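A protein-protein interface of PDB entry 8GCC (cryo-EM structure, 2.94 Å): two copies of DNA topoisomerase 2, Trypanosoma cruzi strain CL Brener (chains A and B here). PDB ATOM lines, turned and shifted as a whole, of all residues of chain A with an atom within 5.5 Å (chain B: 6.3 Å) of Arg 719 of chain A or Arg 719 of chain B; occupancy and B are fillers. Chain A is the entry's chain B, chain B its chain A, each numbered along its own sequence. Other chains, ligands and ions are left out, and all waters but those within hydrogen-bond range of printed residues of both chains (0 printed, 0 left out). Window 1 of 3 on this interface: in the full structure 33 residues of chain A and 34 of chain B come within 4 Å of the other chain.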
ATOM      1  N   LEU A 716      32.466 -24.669  17.268  1.00  0.00           N
ATOM      2  CA  LEU A 716      32.832 -25.787  16.414  1.00  0.00           C
ATOM      3  C   LEU A 716      31.797 -26.901  16.435  1.00  0.00           C
ATOM      4  O   LEU A 716      31.902 -27.836  15.636  1.00  0.00           O
ATOM      5  CB  LEU A 716      34.194 -26.334  16.834  1.00  0.00           C
ATOM      6  CG  LEU A 716      35.359 -25.376  16.589  1.00  0.00           C
ATOM      7  CD1 LEU A 716      36.609 -25.840  17.316  1.00  0.00           C
ATOM      8  CD2 LEU A 716      35.630 -25.234  15.104  1.00  0.00           C
ATOM      9  N   GLY A 717      30.814 -26.833  17.324  1.00  0.00           N
ATOM     10  CA  GLY A 717      29.707 -27.760  17.321  1.00  0.00           C
ATOM     11  C   GLY A 717      28.571 -27.387  16.399  1.00  0.00           C
ATOM     12  O   GLY A 717      27.571 -28.107  16.348  1.00  0.00           O
ATOM     13  N   MET A 718      28.675 -26.276  15.674  1.00  0.00           N
ATOM     14  CA  MET A 718      27.650 -25.939  14.699  1.00  0.00           C
ATOM     15  C   MET A 718      27.674 -26.937  13.554  1.00  0.00           C
ATOM     16  O   MET A 718      28.739 -27.377  13.113  1.00  0.00           O
ATOM     17  CB  MET A 718      27.849 -24.527  14.149  1.00  0.00           C
ATOM     18  CG  MET A 718      26.952 -23.480  14.787  1.00  0.00           C
ATOM     19  SD  MET A 718      27.406 -21.782  14.375  1.00  0.00           S
ATOM     20  CE  MET A 718      28.994 -21.633  15.173  1.00  0.00           C
ATOM     21  N   ARG A 719      26.492 -27.296  13.071  1.00  0.00           N
ATOM     22  CA  ARG A 719      26.398 -28.217  11.953  1.00  0.00           C
ATOM     23  C   ARG A 719      26.805 -27.517  10.663  1.00  0.00           C
ATOM     24  O   ARG A 719      26.806 -26.289  10.562  1.00  0.00           O
ATOM     25  CB  ARG A 719      24.979 -28.771  11.827  1.00  0.00           C
ATOM     26  CG  ARG A 719      24.279 -29.017  13.151  1.00  0.00           C
ATOM     27  CD  ARG A 719      23.699 -30.408  13.223  1.00  0.00           C
ATOM     28  NE  ARG A 719      22.790 -30.548  14.354  1.00  0.00           N
ATOM     29  CZ  ARG A 719      23.079 -31.167  15.492  1.00  0.00           C
ATOM     30  NH1 ARG A 719      24.267 -31.708  15.708  1.00  0.00           N
ATOM     31  NH2 ARG A 719      22.152 -31.238  16.444  1.00  0.00           N
ATOM     32  N   LEU A 720      27.166 -28.320   9.664  1.00  0.00           N
ATOM     33  CA  LEU A 720      27.526 -27.765   8.367  1.00  0.00           C
ATOM     34  C   LEU A 720      26.339 -27.131   7.663  1.00  0.00           C
ATOM     35  O   LEU A 720      26.530 -26.454   6.649  1.00  0.00           O
ATOM     36  CB  LEU A 720      28.139 -28.848   7.482  1.00  0.00           C
ATOM     37  CG  LEU A 720      29.662 -28.792   7.380  1.00  0.00           C
ATOM     38  CD1 LEU A 720      30.291 -29.297   8.657  1.00  0.00           C
ATOM     39  CD2 LEU A 720      30.141 -29.602   6.195  1.00  0.00           C
ATOM     40  N   TRP A 721      25.123 -27.346   8.166  1.00  0.00           N
ATOM     41  CA  TRP A 721      23.965 -26.642   7.632  1.00  0.00           C
ATOM     42  C   TRP A 721      24.126 -25.137   7.789  1.00  0.00           C
ATOM     43  O   TRP A 721      23.751 -24.366   6.898  1.00  0.00           O
ATOM     44  CB  TRP A 721      22.697 -27.111   8.343  1.00  0.00           C
ATOM     45  CG  TRP A 721      21.984 -28.236   7.669  1.00  0.00           C
ATOM     46  CD1 TRP A 721      21.646 -29.435   8.218  1.00  0.00           C
ATOM     47  CD2 TRP A 721      21.506 -28.265   6.319  1.00  0.00           C
ATOM     48  NE1 TRP A 721      20.991 -30.212   7.296  1.00  0.00           N
ATOM     49  CE2 TRP A 721      20.892 -29.516   6.121  1.00  0.00           C
ATOM     50  CE3 TRP A 721      21.539 -27.355   5.260  1.00  0.00           C
ATOM     51  CZ2 TRP A 721      20.318 -29.880   4.907  1.00  0.00           C
ATOM     52  CZ3 TRP A 721      20.970 -27.719   4.057  1.00  0.00           C
ATOM     53  CH2 TRP A 721      20.367 -28.969   3.890  1.00  0.00           C
ATOM     54  N   ASN A 722      24.679 -24.700   8.922  1.00  0.00           N
ATOM     55  CA  ASN A 722      24.762 -23.277   9.221  1.00  0.00           C
ATOM     56  C   ASN A 722      25.682 -22.528   8.270  1.00  0.00           C
ATOM     57  O   ASN A 722      25.632 -21.296   8.232  1.00  0.00           O
ATOM     58  CB  ASN A 722      25.231 -23.074  10.659  1.00  0.00           C
ATOM     59  CG  ASN A 722      24.279 -23.676  11.670  1.00  0.00           C
ATOM     60  OD1 ASN A 722      23.234 -23.107  11.970  1.00  0.00           O
ATOM     61  ND2 ASN A 722      24.636 -24.837  12.198  1.00  0.00           N
ATOM     62  N   LEU A 723      26.519 -23.230   7.511  1.00  0.00           N
ATOM     63  CA  LEU A 723      27.393 -22.586   6.530  1.00  0.00           C
ATOM     64  C   LEU A 723      26.725 -22.515   5.160  1.00  0.00           C
ATOM     65  O   LEU A 723      27.290 -22.906   4.142  1.00  0.00           O
ATOM     66  CB  LEU A 723      28.721 -23.331   6.456  1.00  0.00           C
ATOM     67  CG  LEU A 723      29.784 -22.883   7.457  1.00  0.00           C
ATOM     68  CD1 LEU A 723      29.242 -22.926   8.874  1.00  0.00           C
ATOM     69  CD2 LEU A 723      31.026 -23.747   7.330  1.00  0.00           C
ATOM     70  N   LEU B 716      25.249 -33.007   5.760  1.00  0.00           N
ATOM     71  CA  LEU B 716      25.273 -31.606   6.144  1.00  0.00           C
ATOM     72  C   LEU B 716      24.851 -31.386   7.589  1.00  0.00           C
ATOM     73  O   LEU B 716      24.798 -30.238   8.035  1.00  0.00           O
ATOM     74  CB  LEU B 716      24.370 -30.796   5.213  1.00  0.00           C
ATOM     75  CG  LEU B 716      24.888 -30.649   3.784  1.00  0.00           C
ATOM     76  CD1 LEU B 716      23.782 -30.184   2.859  1.00  0.00           C
ATOM     77  CD2 LEU B 716      26.057 -29.685   3.738  1.00  0.00           C
ATOM     78  N   GLY B 717      24.543 -32.450   8.324  1.00  0.00           N
ATOM     79  CA  GLY B 717      24.185 -32.328   9.721  1.00  0.00           C
ATOM     80  C   GLY B 717      25.310 -32.731  10.651  1.00  0.00           C
ATOM     81  O   GLY B 717      25.077 -32.991  11.834  1.00  0.00           O
ATOM     82  N   MET B 718      26.533 -32.791  10.132  1.00  0.00           N
ATOM     83  CA  MET B 718      27.695 -33.179  10.919  1.00  0.00           C
ATOM     84  C   MET B 718      28.416 -31.925  11.385  1.00  0.00           C
ATOM     85  O   MET B 718      28.724 -31.043  10.579  1.00  0.00           O
ATOM     86  CB  MET B 718      28.647 -34.076  10.124  1.00  0.00           C
ATOM     87  CG  MET B 718      28.954 -33.612   8.711  1.00  0.00           C
ATOM     88  SD  MET B 718      29.768 -34.868   7.698  1.00  0.00           S
ATOM     89  CE  MET B 718      30.644 -35.831   8.927  1.00  0.00           C
ATOM     90  N   ARG B 719      28.684 -31.855  12.684  1.00  0.00           N
ATOM     91  CA  ARG B 719      29.235 -30.651  13.282  1.00  0.00           C
ATOM     92  C   ARG B 719      30.547 -30.263  12.609  1.00  0.00           C
ATOM     93  O   ARG B 719      31.192 -31.063  11.931  1.00  0.00           O
ATOM     94  CB  ARG B 719      29.444 -30.859  14.780  1.00  0.00           C
ATOM     95  CG  ARG B 719      28.160 -31.196  15.525  1.00  0.00           C
ATOM     96  CD  ARG B 719      28.290 -32.439  16.383  1.00  0.00           C
ATOM     97  NE  ARG B 719      28.581 -32.109  17.773  1.00  0.00           N
ATOM     98  N   LEU B 720      30.932 -29.001  12.799  1.00  0.00           N
ATOM     99  CA  LEU B 720      32.177 -28.500  12.233  1.00  0.00           C
ATOM    100  C   LEU B 720      33.402 -29.123  12.881  1.00  0.00           C
ATOM    101  O   LEU B 720      34.510 -28.939  12.371  1.00  0.00           O
ATOM    102  CB  LEU B 720      32.243 -26.979  12.370  1.00  0.00           C
ATOM    103  CG  LEU B 720      31.978 -26.196  11.086  1.00  0.00           C
ATOM    104  CD1 LEU B 720      30.525 -26.313  10.689  1.00  0.00           C
ATOM    105  CD2 LEU B 720      32.366 -24.745  11.265  1.00  0.00           C
ATOM    106  N   TRP B 721      33.232 -29.837  13.993  1.00  0.00           N
ATOM    107  CA  TRP B 721      34.349 -30.563  14.581  1.00  0.00           C
ATOM    108  C   TRP B 721      34.947 -31.542  13.581  1.00  0.00           C
ATOM    109  O   TRP B 721      36.167 -31.738  13.542  1.00  0.00           O
ATOM    110  CB  TRP B 721      33.883 -31.309  15.831  1.00  0.00           C
ATOM    111  CG  TRP B 721      34.049 -30.548  17.105  1.00  0.00           C
ATOM    112  CD1 TRP B 721      33.075 -30.253  18.012  1.00  0.00           C
ATOM    113  CD2 TRP B 721      35.263 -29.998  17.626  1.00  0.00           C
ATOM    114  NE1 TRP B 721      33.606 -29.549  19.064  1.00  0.00           N
ATOM    115  CE2 TRP B 721      34.948 -29.379  18.850  1.00  0.00           C
ATOM    116  CE3 TRP B 721      36.584 -29.967  17.176  1.00  0.00           C
ATOM    117  CZ2 TRP B 721      35.905 -28.735  19.628  1.00  0.00           C
ATOM    118  CZ3 TRP B 721      37.533 -29.327  17.947  1.00  0.00           C
ATOM    119  CH2 TRP B 721      37.190 -28.720  19.160  1.00  0.00           C
ATOM    120  N   ASN B 722      34.099 -32.166  12.761  1.00  0.00           N
ATOM    121  CA  ASN B 722      34.556 -33.211  11.856  1.00  0.00           C
ATOM    122  C   ASN B 722      35.477 -32.685  10.766  1.00  0.00           C
ATOM    123  O   ASN B 722      36.152 -33.485  10.112  1.00  0.00           O
ATOM    124  CB  ASN B 722      33.355 -33.911  11.226  1.00  0.00           C
ATOM    125  CG  ASN B 722      32.469 -34.578  12.254  1.00  0.00           C
ATOM    126  OD1 ASN B 722      32.785 -35.652  12.760  1.00  0.00           O
ATOM    127  ND2 ASN B 722      31.352 -33.943  12.571  1.00  0.00           N
ATOM    128  N   LEU B 723      35.520 -31.373  10.548  1.00  0.00           N
ATOM    129  CA  LEU B 723      36.420 -30.786   9.554  1.00  0.00           C
ATOM    130  C   LEU B 723      37.755 -30.397  10.181  1.00  0.00           C
ATOM    131  O   LEU B 723      38.242 -29.280  10.028  1.00  0.00           O
ATOM    132  CB  LEU B 723      35.750 -29.587   8.897  1.00  0.00           C
ATOM    133  CG  LEU B 723      34.881 -29.903   7.681  1.00  0.00           C
ATOM    134  CD1 LEU B 723      33.835 -30.947   8.022  1.00  0.00           C
ATOM    135  CD2 LEU B 723      34.227 -28.638   7.156  1.00  0.00           C
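O of Leu 716 of chain B lies within hydrogen-bond range of N of Trp 721 of chain A, 2.9 Å away. N of Leu 720 of chain B is in hydrogen-bond range of O of Met 718 of chain A (2.7 Å). O of Met 718 of chain B lies close to N of Leu 720 of chain A (3.3 Å). O of Leu 716 of chain B sits at hydrogen-bond distance from N of Leu 720 of chain A (3.5 Å). The backbone carbonyl oxygen of Leu 716 of chain A lies within hydrogen-bond range of the backbone NH of Leu 720 of chain B. The backbone carbonyl oxygen (O) of Leu 716 of chain A sits at hydrogen-bond distance from the backbone NH (N) of Trp 721 of chain B, 2.9 Å away.
ND2 of Asn 722 of chain A lies within hydrogen-bond range of O of Arg 719 of chain A, 3.1 Å away. The backbone carbonyl oxygen of Arg 719 of chain B sits at hydrogen-bond distance from the side-chain amide nitrogen of Asn 722 of chain B, at 3.0 Å.
Leu 716 of chain A touches Arg 719 of chain B. Arg 719 of chain B touches Gly 717 of chain A. CA of Arg 719 of chain B touches O of Met 718 of chain A (3.3 Å). Gly 717 of chain B touches Arg 719 of chain A. CA of Arg 719 of chain A touches O of Met 718 of chain B, 3.9 Å away. Arg 719 of chain A touches Arg 719 of chain B (NH1 to CG, 3.9 Å). Leu 720 of chain B touches Arg 719 of chain A (CD1 to O, 3.7 Å). Arg 719 of chain B touches Leu 720 of chain A. Leu 720 of chain A touches Leu 720 of chain B. CD1 of Leu 720 of chain A touches CD1 of Leu 723 of chain B, at 3.96 Å.
Of the printed residues of chain B, Leu 716 of chain A touches Arg 719, Leu 720 and Trp 721. Printed residues of chain B within 4 Å of Gly 717 of chain A: Arg 719 (3.3 Å). Printed residues of chain B within 4 Å of Met 718 of chain A: Arg 719 and Leu 720. Asn 722 of chain A touches none of the printed residues of chain B. Leu 723 of chain A touches none of the printed residues of chain B. Of the printed residues of chain A, Arg 719 of chain B touches Leu 716, Gly 717, Met 718, Arg 719 and Leu 720. Of the printed residues of chain A, Trp 721 of chain B touches Leu 716 (2.9 Å). Of the printed residues of chain A, Leu 723 of chain B touches Leu 720 (3.96 Å). The nearest printed residue of chain A that does not touch Arg 719 of chain B is Trp 721 of chain A (7.3 Å).
Hydrophobic or aromatic side chains of chain B that line the printed part of chain A: Leu 716, Leu 720, Trp 721 and Leu 723. Printed residues of chain A that touch a printed residue of chain B: Leu 716, Gly 717, Met 718, Arg 719, Leu 720 and Trp 721. Hydrophobic or aromatic side chains of chain A within 4 Å of the printed part of chain B: Leu 716, Leu 720 and Trp 721.
Leu 716 of chain A touches Arg 719 of chain B, but with the chains exchanged Arg 719 of chain A does not touch Leu 716 of chain B (4.1 Å). Leu 716 of chain A touches Trp 721 of chain B, and with the chains exchanged Trp 721 of chain A touches Leu 716 of chain B. Leu 720 of chain B touches its own counterpart, Leu 720 of chain A. Leu 720 of chain A touches Leu 723 of chain B, but with the chains exchanged Leu 723 of chain A does not touch Leu 720 of chain B (4.1 Å). Of the 16 pairs that touch across the chains among the printed residues, 14 have their exchanged pair printed and touching as well.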
